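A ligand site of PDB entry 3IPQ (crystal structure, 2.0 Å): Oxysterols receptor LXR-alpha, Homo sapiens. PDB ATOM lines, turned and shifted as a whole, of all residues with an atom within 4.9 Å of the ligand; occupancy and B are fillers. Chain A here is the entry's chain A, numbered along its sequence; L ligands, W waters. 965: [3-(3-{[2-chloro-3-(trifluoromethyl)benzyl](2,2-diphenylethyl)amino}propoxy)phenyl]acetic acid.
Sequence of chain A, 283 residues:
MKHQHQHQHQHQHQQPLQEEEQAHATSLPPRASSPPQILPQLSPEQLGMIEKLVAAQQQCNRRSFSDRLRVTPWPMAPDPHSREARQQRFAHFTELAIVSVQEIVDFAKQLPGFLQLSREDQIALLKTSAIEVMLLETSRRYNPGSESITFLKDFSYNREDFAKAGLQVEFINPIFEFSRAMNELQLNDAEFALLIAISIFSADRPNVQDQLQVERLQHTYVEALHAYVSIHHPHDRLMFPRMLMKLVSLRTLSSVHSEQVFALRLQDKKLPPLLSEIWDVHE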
ATOM      1  N   PHE A  90     -31.807  -5.768  14.091  1.00  0.00           N
ATOM      2  CA  PHE A  90     -30.573  -6.527  14.272  1.00  0.00           C
ATOM      3  C   PHE A  90     -30.613  -7.859  13.541  1.00  0.00           C
ATOM      4  O   PHE A  90     -29.618  -8.276  12.948  1.00  0.00           O
ATOM      5  CB  PHE A  90     -30.306  -6.757  15.745  1.00  0.00           C
ATOM      6  CG  PHE A  90     -28.936  -7.293  16.036  1.00  0.00           C
ATOM      7  CD1 PHE A  90     -27.825  -6.457  16.031  1.00  0.00           C
ATOM      8  CD2 PHE A  90     -28.759  -8.636  16.315  1.00  0.00           C
ATOM      9  CE1 PHE A  90     -26.552  -6.960  16.298  1.00  0.00           C
ATOM     10  CE2 PHE A  90     -27.491  -9.141  16.594  1.00  0.00           C
ATOM     11  CZ  PHE A  90     -26.387  -8.297  16.580  1.00  0.00           C
ATOM     12  N   PHE A  93     -30.265  -7.027   9.690  1.00  0.00           N
ATOM     13  CA  PHE A  93     -28.848  -6.677   9.413  1.00  0.00           C
ATOM     14  C   PHE A  93     -27.912  -7.879   9.487  1.00  0.00           C
ATOM     15  O   PHE A  93     -27.145  -8.110   8.568  1.00  0.00           O
ATOM     16  CB  PHE A  93     -28.369  -5.571  10.362  1.00  0.00           C
ATOM     17  CG  PHE A  93     -28.825  -4.166   9.989  1.00  0.00           C
ATOM     18  CD1 PHE A  93     -29.191  -3.824   8.675  1.00  0.00           C
ATOM     19  CD2 PHE A  93     -28.860  -3.177  10.952  1.00  0.00           C
ATOM     20  CE1 PHE A  93     -29.595  -2.530   8.360  1.00  0.00           C
ATOM     21  CE2 PHE A  93     -29.296  -1.887  10.638  1.00  0.00           C
ATOM     22  CZ  PHE A  93     -29.660  -1.578   9.348  1.00  0.00           C
ATOM     23  N   THR A  94     -28.007  -8.678  10.560  1.00  0.00           N
ATOM     24  CA  THR A  94     -27.197  -9.907  10.668  1.00  0.00           C
ATOM     25  C   THR A  94     -27.495 -10.899   9.540  1.00  0.00           C
ATOM     26  O   THR A  94     -26.612 -11.627   9.093  1.00  0.00           O
ATOM     27  CB  THR A  94     -27.294 -10.587  12.036  1.00  0.00           C
ATOM     28  OG1 THR A  94     -28.645 -10.973  12.315  1.00  0.00           O
ATOM     29  CG2 THR A  94     -26.775  -9.668  13.129  1.00  0.00           C
ATOM     30  N   LEU A  96     -28.439  -9.951   6.445  1.00  0.00           N
ATOM     31  CA  LEU A  96     -27.783  -9.372   5.274  1.00  0.00           C
ATOM     32  C   LEU A  96     -26.268  -9.652   5.288  1.00  0.00           C
ATOM     33  O   LEU A  96     -25.687  -9.899   4.263  1.00  0.00           O
ATOM     34  CB  LEU A  96     -27.992  -7.867   5.210  1.00  0.00           C
ATOM     35  CG  LEU A  96     -29.371  -7.311   4.888  1.00  0.00           C
ATOM     36  CD1 LEU A  96     -29.420  -5.815   5.197  1.00  0.00           C
ATOM     37  CD2 LEU A  96     -29.691  -7.604   3.448  1.00  0.00           C
ATOM     38  N   ALA A  97     -25.645  -9.548   6.457  1.00  0.00           N
ATOM     39  CA  ALA A  97     -24.245  -9.868   6.672  1.00  0.00           C
ATOM     40  C   ALA A  97     -23.912 -11.307   6.284  1.00  0.00           C
ATOM     41  O   ALA A  97     -22.839 -11.577   5.713  1.00  0.00           O
ATOM     42  CB  ALA A  97     -23.875  -9.607   8.110  1.00  0.00           C
ATOM     43  N   VAL A  99     -25.573 -13.033   3.995  1.00  0.00           N
ATOM     44  CA  VAL A  99     -25.577 -12.980   2.528  1.00  0.00           C
ATOM     45  C   VAL A  99     -24.210 -12.454   2.006  1.00  0.00           C
ATOM     46  O   VAL A  99     -23.639 -13.043   1.106  1.00  0.00           O
ATOM     47  CB  VAL A  99     -26.719 -12.116   1.956  1.00  0.00           C
ATOM     48  CG1 VAL A  99     -26.630 -12.015   0.390  1.00  0.00           C
ATOM     49  CG2 VAL A  99     -28.065 -12.673   2.401  1.00  0.00           C
ATOM     50  N   SER A 100     -23.691 -11.391   2.607  1.00  0.00           N
ATOM     51  CA  SER A 100     -22.385 -10.876   2.190  1.00  0.00           C
ATOM     52  C   SER A 100     -21.272 -11.913   2.378  1.00  0.00           C
ATOM     53  O   SER A 100     -20.491 -12.160   1.446  1.00  0.00           O
ATOM     54  CB  SER A 100     -22.027  -9.597   2.948  1.00  0.00           C
ATOM     55  OG  SER A 100     -20.745  -9.118   2.575  1.00  0.00           O
ATOM     56  N   GLU A 103     -21.384 -14.523  -0.351  1.00  0.00           N
ATOM     57  CA  GLU A 103     -20.847 -13.932  -1.569  1.00  0.00           C
ATOM     58  C   GLU A 103     -19.312 -13.817  -1.531  1.00  0.00           C
ATOM     59  O   GLU A 103     -18.668 -14.047  -2.525  1.00  0.00           O
ATOM     60  CB  GLU A 103     -21.461 -12.541  -1.792  1.00  0.00           C
ATOM     61  CG  GLU A 103     -22.951 -12.570  -2.035  1.00  0.00           C
ATOM     62  CD  GLU A 103     -23.556 -11.198  -2.471  1.00  0.00           C
ATOM     63  OE1 GLU A 103     -22.962 -10.096  -2.206  1.00  0.00           O
ATOM     64  OE2 GLU A 103     -24.664 -11.278  -3.068  1.00  0.00           O
ATOM     65  N   ILE A 131     -14.450  -9.455   7.299  1.00  0.00           N
ATOM     66  CA  ILE A 131     -14.922  -8.127   7.734  1.00  0.00           C
ATOM     67  C   ILE A 131     -14.402  -7.006   6.824  1.00  0.00           C
ATOM     68  O   ILE A 131     -15.120  -6.065   6.473  1.00  0.00           O
ATOM     69  CB  ILE A 131     -14.605  -7.849   9.241  1.00  0.00           C
ATOM     70  CG1 ILE A 131     -15.378  -6.606   9.701  1.00  0.00           C
ATOM     71  CG2 ILE A 131     -13.083  -7.707   9.524  1.00  0.00           C
ATOM     72  CD1 ILE A 131     -16.926  -6.772   9.684  1.00  0.00           C
ATOM     73  N   MET A 134     -16.258  -7.103   3.596  1.00  0.00           N
ATOM     74  CA  MET A 134     -17.615  -6.576   3.873  1.00  0.00           C
ATOM     75  C   MET A 134     -17.604  -5.029   3.944  1.00  0.00           C
ATOM     76  O   MET A 134     -18.488  -4.358   3.434  1.00  0.00           O
ATOM     77  CB  MET A 134     -18.166  -7.122   5.176  1.00  0.00           C
ATOM     78  CG  MET A 134     -18.522  -8.577   5.146  1.00  0.00           C
ATOM     79  SD  MET A 134     -19.377  -9.153   6.659  1.00  0.00           S
ATOM     80  CE  MET A 134     -20.683  -7.959   6.624  1.00  0.00           C
ATOM     81  N   LEU A 135     -16.556  -4.482   4.542  1.00  0.00           N
ATOM     82  CA  LEU A 135     -16.365  -3.051   4.630  1.00  0.00           C
ATOM     83  C   LEU A 135     -16.130  -2.437   3.234  1.00  0.00           C
ATOM     84  O   LEU A 135     -16.715  -1.414   2.903  1.00  0.00           O
ATOM     85  CB  LEU A 135     -15.248  -2.731   5.611  1.00  0.00           C
ATOM     86  CG  LEU A 135     -15.598  -2.872   7.088  1.00  0.00           C
ATOM     87  CD1 LEU A 135     -14.325  -2.893   7.928  1.00  0.00           C
ATOM     88  CD2 LEU A 135     -16.549  -1.743   7.493  1.00  0.00           C
ATOM     89  N   GLU A 137     -17.135  -3.777   0.324  1.00  0.00           N
ATOM     90  CA  GLU A 137     -18.444  -3.914  -0.317  1.00  0.00           C
ATOM     91  C   GLU A 137     -19.475  -2.858   0.155  1.00  0.00           C
ATOM     92  O   GLU A 137     -20.240  -2.317  -0.635  1.00  0.00           O
ATOM     93  CB  GLU A 137     -19.013  -5.315  -0.070  1.00  0.00           C
ATOM     94  CG  GLU A 137     -18.274  -6.431  -0.734  1.00  0.00           C
ATOM     95  CD  GLU A 137     -18.376  -6.408  -2.281  1.00  0.00           C
ATOM     96  OE1 GLU A 137     -18.829  -5.422  -2.895  1.00  0.00           O
ATOM     97  OE2 GLU A 137     -17.987  -7.414  -2.894  1.00  0.00           O
ATOM     98  N   THR A 138     -19.476  -2.563   1.437  1.00  0.00           N
ATOM     99  CA  THR A 138     -20.310  -1.509   2.023  1.00  0.00           C
ATOM    100  C   THR A 138     -19.958  -0.097   1.497  1.00  0.00           C
ATOM    101  O   THR A 138     -20.847   0.696   1.187  1.00  0.00           O
ATOM    102  CB  THR A 138     -20.226  -1.574   3.591  1.00  0.00           C
ATOM    103  OG1 THR A 138     -20.797  -2.808   4.043  1.00  0.00           O
ATOM    104  CG2 THR A 138     -20.922  -0.385   4.308  1.00  0.00           C
ATOM    105  N   ARG A 141     -21.396   0.608  -1.778  1.00  0.00           N
ATOM    106  CA  ARG A 141     -22.839   0.765  -1.760  1.00  0.00           C
ATOM    107  C   ARG A 141     -23.315   2.071  -1.119  1.00  0.00           C
ATOM    108  O   ARG A 141     -24.504   2.258  -0.861  1.00  0.00           O
ATOM    109  CB  ARG A 141     -23.426  -0.434  -1.031  1.00  0.00           C
ATOM    110  CG  ARG A 141     -23.386  -1.678  -1.904  1.00  0.00           C
ATOM    111  CD  ARG A 141     -23.546  -2.916  -1.059  1.00  0.00           C
ATOM    112  NE  ARG A 141     -23.658  -4.159  -1.808  1.00  0.00           N
ATOM    113  CZ  ARG A 141     -22.671  -4.729  -2.487  1.00  0.00           C
ATOM    114  NH1 ARG A 141     -21.487  -4.165  -2.582  1.00  0.00           N
ATOM    115  NH2 ARG A 141     -22.889  -5.884  -3.094  1.00  0.00           N
ATOM    116  N   ILE A 149     -26.504   3.853   2.862  1.00  0.00           N
ATOM    117  CA  ILE A 149     -25.914   2.654   2.256  1.00  0.00           C
ATOM    118  C   ILE A 149     -27.041   1.743   1.820  1.00  0.00           C
ATOM    119  O   ILE A 149     -27.919   1.465   2.609  1.00  0.00           O
ATOM    120  CB  ILE A 149     -25.028   1.873   3.244  1.00  0.00           C
ATOM    121  CG1 ILE A 149     -23.861   2.756   3.745  1.00  0.00           C
ATOM    122  CG2 ILE A 149     -24.528   0.546   2.577  1.00  0.00           C
ATOM    123  CD1 ILE A 149     -23.330   2.367   5.126  1.00  0.00           C
ATOM    124  N   THR A 150     -26.967   1.247   0.599  1.00  0.00           N
ATOM    125  CA  THR A 150     -27.994   0.377   0.019  1.00  0.00           C
ATOM    126  C   THR A 150     -27.519  -1.075  -0.076  1.00  0.00           C
ATOM    127  O   THR A 150     -26.556  -1.369  -0.778  1.00  0.00           O
ATOM    128  CB  THR A 150     -28.377   0.850  -1.421  1.00  0.00           C
ATOM    129  OG1 THR A 150     -28.905   2.191  -1.360  1.00  0.00           O
ATOM    130  CG2 THR A 150     -29.385  -0.085  -2.095  1.00  0.00           C
ATOM    131  N   PHE A 151     -28.253  -1.975   0.585  1.00  0.00           N
ATOM    132  CA  PHE A 151     -28.007  -3.414   0.522  1.00  0.00           C
ATOM    133  C   PHE A 151     -29.073  -4.111  -0.371  1.00  0.00           C
ATOM    134  O   PHE A 151     -30.251  -3.708  -0.394  1.00  0.00           O
ATOM    135  CB  PHE A 151     -27.961  -4.019   1.929  1.00  0.00           C
ATOM    136  CG  PHE A 151     -26.944  -3.357   2.864  1.00  0.00           C
ATOM    137  CD1 PHE A 151     -25.585  -3.466   2.625  1.00  0.00           C
ATOM    138  CD2 PHE A 151     -27.366  -2.655   3.987  1.00  0.00           C
ATOM    139  CE1 PHE A 151     -24.660  -2.865   3.460  1.00  0.00           C
ATOM    140  CE2 PHE A 151     -26.459  -2.052   4.838  1.00  0.00           C
ATOM    141  CZ  PHE A 151     -25.087  -2.154   4.583  1.00  0.00           C
ATOM    142  N   LEU A 152     -28.616  -5.111  -1.135  1.00  0.00           N
ATOM    143  CA  LEU A 152     -29.430  -5.923  -2.036  1.00  0.00           C
ATOM    144  C   LEU A 152     -30.266  -5.076  -2.995  1.00  0.00           C
ATOM    145  O   LEU A 152     -31.381  -5.456  -3.345  1.00  0.00           O
ATOM    146  CB  LEU A 152     -30.320  -6.879  -1.243  1.00  0.00           C
ATOM    147  CG  LEU A 152     -29.578  -7.878  -0.321  1.00  0.00           C
ATOM    148  CD1 LEU A 152     -30.569  -8.693   0.447  1.00  0.00           C
ATOM    149  CD2 LEU A 152     -28.648  -8.756  -1.139  1.00  0.00           C
ATOM    150  N   PHE A 162     -28.860   2.334  11.801  1.00  0.00           N
ATOM    151  CA  PHE A 162     -27.890   1.422  12.415  1.00  0.00           C
ATOM    152  C   PHE A 162     -27.888   1.553  13.926  1.00  0.00           C
ATOM    153  O   PHE A 162     -27.838   0.542  14.592  1.00  0.00           O
ATOM    154  CB  PHE A 162     -26.484   1.627  11.809  1.00  0.00           C
ATOM    155  CG  PHE A 162     -26.392   1.206  10.362  1.00  0.00           C
ATOM    156  CD1 PHE A 162     -26.358  -0.132  10.030  1.00  0.00           C
ATOM    157  CD2 PHE A 162     -26.369   2.145   9.340  1.00  0.00           C
ATOM    158  CE1 PHE A 162     -26.280  -0.511   8.721  1.00  0.00           C
ATOM    159  CE2 PHE A 162     -26.304   1.771   8.035  1.00  0.00           C
ATOM    160  CZ  PHE A 162     -26.251   0.431   7.719  1.00  0.00           C
ATOM    161  N   LEU A 167     -26.373  -0.979  17.407  1.00  0.00           N
ATOM    162  CA  LEU A 167     -24.940  -0.950  17.076  1.00  0.00           C
ATOM    163  C   LEU A 167     -24.363   0.281  17.734  1.00  0.00           C
ATOM    164  O   LEU A 167     -25.047   1.292  17.862  1.00  0.00           O
ATOM    165  CB  LEU A 167     -24.747  -0.924  15.536  1.00  0.00           C
ATOM    166  CG  LEU A 167     -25.405  -2.112  14.814  1.00  0.00           C
ATOM    167  CD1 LEU A 167     -25.214  -2.111  13.331  1.00  0.00           C
ATOM    168  CD2 LEU A 167     -24.930  -3.409  15.434  1.00  0.00           C
ATOM    169  N   PHE A 171     -18.718   2.192  16.325  1.00  0.00           N
ATOM    170  CA  PHE A 171     -18.679   1.257  15.196  1.00  0.00           C
ATOM    171  C   PHE A 171     -19.222   1.953  13.987  1.00  0.00           C
ATOM    172  O   PHE A 171     -18.567   2.006  12.947  1.00  0.00           O
ATOM    173  CB  PHE A 171     -19.580   0.062  15.542  1.00  0.00           C
ATOM    174  CG  PHE A 171     -19.591  -1.057  14.544  1.00  0.00           C
ATOM    175  CD1 PHE A 171     -18.432  -1.729  14.211  1.00  0.00           C
ATOM    176  CD2 PHE A 171     -20.803  -1.518  14.023  1.00  0.00           C
ATOM    177  CE1 PHE A 171     -18.466  -2.808  13.323  1.00  0.00           C
ATOM    178  CE2 PHE A 171     -20.820  -2.602  13.173  1.00  0.00           C
ATOM    179  CZ  PHE A 171     -19.622  -3.233  12.811  1.00  0.00           C
ATOM    180  N   ILE A 172     -20.431   2.511  14.137  1.00  0.00           N
ATOM    181  CA  ILE A 172     -21.121   3.189  13.042  1.00  0.00           C
ATOM    182  C   ILE A 172     -20.292   4.307  12.443  1.00  0.00           C
ATOM    183  O   ILE A 172     -20.198   4.405  11.225  1.00  0.00           O
ATOM    184  CB  ILE A 172     -22.510   3.760  13.474  1.00  0.00           C
ATOM    185  CG1 ILE A 172     -23.474   2.643  13.906  1.00  0.00           C
ATOM    186  CG2 ILE A 172     -23.146   4.598  12.323  1.00  0.00           C
ATOM    187  CD1 ILE A 172     -24.590   3.107  14.884  1.00  0.00           C
ATOM    188  N   ILE A 175     -17.260   3.512  10.143  1.00  0.00           N
ATOM    189  CA  ILE A 175     -17.677   2.857   8.881  1.00  0.00           C
ATOM    190  C   ILE A 175     -18.202   3.881   7.916  1.00  0.00           C
ATOM    191  O   ILE A 175     -17.837   3.885   6.703  1.00  0.00           O
ATOM    192  CB  ILE A 175     -18.651   1.687   9.132  1.00  0.00           C
ATOM    193  CG1 ILE A 175     -17.922   0.600   9.909  1.00  0.00           C
ATOM    194  CG2 ILE A 175     -19.168   1.132   7.796  1.00  0.00           C
ATOM    195  CD1 ILE A 175     -18.803  -0.402  10.576  1.00  0.00           C
ATOM    196  N   PHE A 176     -18.999   4.824   8.428  1.00  0.00           N
ATOM    197  CA  PHE A 176     -19.427   5.966   7.555  1.00  0.00           C
ATOM    198  C   PHE A 176     -18.267   6.856   7.104  1.00  0.00           C
ATOM    199  O   PHE A 176     -18.228   7.278   5.964  1.00  0.00           O
ATOM    200  CB  PHE A 176     -20.577   6.794   8.197  1.00  0.00           C
ATOM    201  CG  PHE A 176     -21.919   6.228   7.911  1.00  0.00           C
ATOM    202  CD1 PHE A 176     -22.454   5.259   8.725  1.00  0.00           C
ATOM    203  CD2 PHE A 176     -22.642   6.648   6.803  1.00  0.00           C
ATOM    204  CE1 PHE A 176     -23.687   4.699   8.455  1.00  0.00           C
ATOM    205  CE2 PHE A 176     -23.894   6.114   6.515  1.00  0.00           C
ATOM    206  CZ  PHE A 176     -24.423   5.124   7.350  1.00  0.00           C
ATOM    207  N   HIS A 257     -14.364  -3.348  14.666  1.00  0.00           N
ATOM    208  CA  HIS A 257     -15.305  -4.454  14.591  1.00  0.00           C
ATOM    209  C   HIS A 257     -15.187  -5.477  15.723  1.00  0.00           C
ATOM    210  O   HIS A 257     -16.217  -5.869  16.279  1.00  0.00           O
ATOM    211  CB  HIS A 257     -15.229  -5.153  13.244  1.00  0.00           C
ATOM    212  CG  HIS A 257     -15.984  -6.450  13.202  1.00  0.00           C
ATOM    213  ND1 HIS A 257     -15.355  -7.673  13.275  1.00  0.00           N
ATOM    214  CD2 HIS A 257     -17.308  -6.708  13.131  1.00  0.00           C
ATOM    215  CE1 HIS A 257     -16.263  -8.633  13.226  1.00  0.00           C
ATOM    216  NE2 HIS A 257     -17.457  -8.069  13.149  1.00  0.00           N
ATOM    217  N   GLN A 260     -16.964  -4.120  18.720  1.00  0.00           N
ATOM    218  CA  GLN A 260     -18.405  -4.243  18.609  1.00  0.00           C
ATOM    219  C   GLN A 260     -18.867  -5.672  18.887  1.00  0.00           C
ATOM    220  O   GLN A 260     -19.933  -5.897  19.499  1.00  0.00           O
ATOM    221  CB  GLN A 260     -18.844  -3.820  17.204  1.00  0.00           C
ATOM    222  CG  GLN A 260     -20.322  -4.018  16.902  1.00  0.00           C
ATOM    223  CD  GLN A 260     -21.216  -3.126  17.770  1.00  0.00           C
ATOM    224  OE1 GLN A 260     -21.631  -2.052  17.335  1.00  0.00           O
ATOM    225  NE2 GLN A 260     -21.532  -3.581  18.973  1.00  0.00           N
ATOM    226  N   VAL A 261     -18.100  -6.653  18.432  1.00  0.00           N
ATOM    227  CA  VAL A 261     -18.446  -8.048  18.657  1.00  0.00           C
ATOM    228  C   VAL A 261     -18.399  -8.337  20.156  1.00  0.00           C
ATOM    229  O   VAL A 261     -19.267  -9.041  20.713  1.00  0.00           O
ATOM    230  CB  VAL A 261     -17.533  -9.001  17.853  1.00  0.00           C
ATOM    231  CG1 VAL A 261     -17.585 -10.418  18.418  1.00  0.00           C
ATOM    232  CG2 VAL A 261     -17.924  -8.993  16.361  1.00  0.00           C
ATOM    233  N   LEU A 264     -21.457  -6.777  21.851  1.00  0.00           N
ATOM    234  CA  LEU A 264     -22.652  -7.575  21.626  1.00  0.00           C
ATOM    235  C   LEU A 264     -22.753  -8.737  22.624  1.00  0.00           C
ATOM    236  O   LEU A 264     -23.855  -9.070  23.069  1.00  0.00           O
ATOM    237  CB  LEU A 264     -22.729  -8.098  20.194  1.00  0.00           C
ATOM    238  CG  LEU A 264     -22.950  -7.079  19.064  1.00  0.00           C
ATOM    239  CD1 LEU A 264     -22.932  -7.804  17.718  1.00  0.00           C
ATOM    240  CD2 LEU A 264     -24.235  -6.259  19.222  1.00  0.00           C
ATOM    241  N   LEU A 271     -25.100 -13.505  17.833  1.00  0.00           N
ATOM    242  CA  LEU A 271     -24.763 -13.538  16.411  1.00  0.00           C
ATOM    243  C   LEU A 271     -25.309 -14.848  15.856  1.00  0.00           C
ATOM    244  O   LEU A 271     -25.237 -15.892  16.508  1.00  0.00           O
ATOM    245  CB  LEU A 271     -23.237 -13.450  16.211  1.00  0.00           C
ATOM    246  CG  LEU A 271     -22.570 -12.076  16.337  1.00  0.00           C
ATOM    247  CD1 LEU A 271     -21.067 -12.173  16.091  1.00  0.00           C
ATOM    248  CD2 LEU A 271     -23.196 -11.097  15.358  1.00  0.00           C
ATOM    249  N   TRP A 279     -16.401 -14.828  13.875  1.00  0.00           N
ATOM    250  CA  TRP A 279     -16.067 -13.675  14.751  1.00  0.00           C
ATOM    251  C   TRP A 279     -16.047 -13.845  16.267  1.00  0.00           C
ATOM    252  O   TRP A 279     -15.275 -13.175  16.943  1.00  0.00           O
ATOM    253  CB  TRP A 279     -17.003 -12.496  14.435  1.00  0.00           C
ATOM    254  CG  TRP A 279     -16.866 -11.993  13.010  1.00  0.00           C
ATOM    255  CD1 TRP A 279     -15.740 -12.030  12.226  1.00  0.00           C
ATOM    256  CD2 TRP A 279     -17.886 -11.382  12.223  1.00  0.00           C
ATOM    257  NE1 TRP A 279     -16.006 -11.458  11.002  1.00  0.00           N
ATOM    258  CE2 TRP A 279     -17.310 -11.047  10.967  1.00  0.00           C
ATOM    259  CE3 TRP A 279     -19.226 -11.044  12.463  1.00  0.00           C
ATOM    260  CZ2 TRP A 279     -18.040 -10.446   9.947  1.00  0.00           C
ATOM    261  CZ3 TRP A 279     -19.957 -10.433  11.452  1.00  0.00           C
ATOM    262  CH2 TRP A 279     -19.360 -10.133  10.204  1.00  0.00           C
HETATM  263  O37 965 L   1     -25.824  -5.656  -0.701  1.00  0.00           O
HETATM  264  C35 965 L   1     -25.463  -6.823  -0.948  1.00  0.00           C
HETATM  265  O36 965 L   1     -25.401  -7.239  -2.099  1.00  0.00           O
HETATM  266  C34 965 L   1     -25.069  -7.803   0.130  1.00  0.00           C
HETATM  267  C32 965 L   1     -24.334  -7.138   1.254  1.00  0.00           C
HETATM  268  C31 965 L   1     -23.059  -6.602   1.025  1.00  0.00           C
HETATM  269  C30 965 L   1     -22.381  -5.981   2.067  1.00  0.00           C
HETATM  270  C29 965 L   1     -22.933  -5.931   3.347  1.00  0.00           C
HETATM  271  C28 965 L   1     -24.228  -6.464   3.561  1.00  0.00           C
HETATM  272  O27 965 L   1     -24.831  -6.457   4.778  1.00  0.00           O
HETATM  273  C26 965 L   1     -24.347  -5.811   5.956  1.00  0.00           C
HETATM  274  C25 965 L   1     -25.509  -5.454   6.865  1.00  0.00           C
HETATM  275  C17 965 L   1     -25.199  -4.292   7.779  1.00  0.00           C
HETATM  276  N09 965 L   1     -24.345  -4.587   8.925  1.00  0.00           N
HETATM  277  C16 965 L   1     -24.324  -5.950   9.502  1.00  0.00           C
HETATM  278  C18 965 L   1     -23.102  -6.334  10.303  1.00  0.00           C
HETATM  279  C23 965 L   1     -21.915  -6.470   9.615  1.00  0.00           C
HETATM  280  C22 965 L   1     -20.775  -6.832  10.293  1.00  0.00           C
HETATM  281  C21 965 L   1     -20.821  -7.081  11.660  1.00  0.00           C
HETATM  282  C20 965 L   1     -22.010  -6.947  12.369  1.00  0.00           C
HETATM  283  C19 965 L   1     -23.161  -6.578  11.674  1.00  0.00           C
HETATM  284 CL4  965 L   1     -24.720  -6.437  12.559  1.00  0.00          CL
HETATM  285  C39 965 L   1     -22.033  -7.213  13.868  1.00  0.00           C
HETATM  286  F41 965 L   1     -23.006  -8.092  14.055  1.00  0.00           F
HETATM  287  F40 965 L   1     -20.906  -7.726  14.323  1.00  0.00           F
HETATM  288  F42 965 L   1     -22.263  -6.082  14.563  1.00  0.00           F
HETATM  289  C08 965 L   1     -23.690  -3.453   9.601  1.00  0.00           C
HETATM  290  C07 965 L   1     -22.879  -2.558   8.618  1.00  0.00           C
HETATM  291  C01 965 L   1     -21.535  -3.169   8.355  1.00  0.00           C
HETATM  292  C02 965 L   1     -21.242  -3.582   7.073  1.00  0.00           C
HETATM  293  C03 965 L   1     -19.998  -4.152   6.817  1.00  0.00           C
HETATM  294  C04 965 L   1     -19.065  -4.327   7.829  1.00  0.00           C
HETATM  295  C05 965 L   1     -19.357  -3.914   9.110  1.00  0.00           C
HETATM  296  C06 965 L   1     -20.599  -3.321   9.374  1.00  0.00           C
HETATM  297  C10 965 L   1     -22.696  -1.172   9.116  1.00  0.00           C
HETATM  298  C15 965 L   1     -22.624  -0.147   8.175  1.00  0.00           C
HETATM  299  C14 965 L   1     -22.490   1.166   8.580  1.00  0.00           C
HETATM  300  C13 965 L   1     -22.394   1.481   9.923  1.00  0.00           C
HETATM  301  C12 965 L   1     -22.454   0.461  10.870  1.00  0.00           C
HETATM  302  C11 965 L   1     -22.622  -0.856  10.466  1.00  0.00           C
HETATM  303  C33 965 L   1     -24.890  -7.089   2.525  1.00  0.00           C
HETATM  304  O   HOH W   1     -26.090  -5.378  -3.726  1.00  0.00           O
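O37 of the ligand is in salt-bridge range of NE of Arg 141 (2.9 Å).
O37 of the ligand lies within hydrogen-bond range of N of Leu 152, at 2.9 Å.
O of Phe 90 is in hydrogen-bond range of OG1 of Thr 94, at 2.9 Å.
The side-chain hydroxyl (OG1) of Thr 138 sits at hydrogen-bond distance from the backbone carbonyl oxygen (O) of Met 134.
N of Thr 150 lies within hydrogen-bond range of O of Arg 141, at 3.0 Å.
The guanidinium group (NH1) of Arg 141 is in salt-bridge range of the side-chain carboxylate (OE1) of Glu 137 (3.0 Å).
Merely in contact with the ligand: Phe 93 (3.6 Å), Thr 94 (3.9 Å), Leu 96 (3.4 Å), Ala 97 (3.6 Å), Ser 100 (3.6 Å), Glu 103 (3.8 Å), Ile 131 (3.7 Å), Met 134 (3.6 Å), Leu 135 (3.6 Å), Thr 138 (3.2 Å), Ile 149 (3.8 Å), Phe 151 (3.4 Å), Phe 162 (3.7 Å), Leu 167 (3.9 Å), Phe 171 (3.6 Å), Ile 172 (3.7 Å), Ile 175 (3.4 Å), Phe 176 (3.7 Å), His 257 (3.7 Å), Gln 260 (3.7 Å), Val 261 (3.8 Å), Leu 264 (3.7 Å), Leu 271 (3.3 Å) and Trp 279 (3.5 Å).
Hydrophobic or aromatic side chains that line the ligand: Leu 96, Ala 97, Ile 131, Met 134, Leu 135, Ile 149, Phe 151, Leu 152, Phe 162, Leu 167, Phe 171, Ile 172, Ile 175, Phe 176, His 257, Val 261, Leu 264, Leu 271 and Trp 279.
26 residues have an atom within 4 Å of the ligand: Phe 93, Thr 94, Leu 96, Ala 97, Ser 100, Glu 103, Ile 131, Met 134, Leu 135, Thr 138, Arg 141, Ile 149, Phe 151, Leu 152, Phe 162, Leu 167, Phe 171, Ile 172, Ile 175, Phe 176, His 257, Gln 260, Val 261, Leu 264, Leu 271 and Trp 279.
Water W1 lies within hydrogen-bond range of O36 of the ligand and NH2 of Arg 141.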
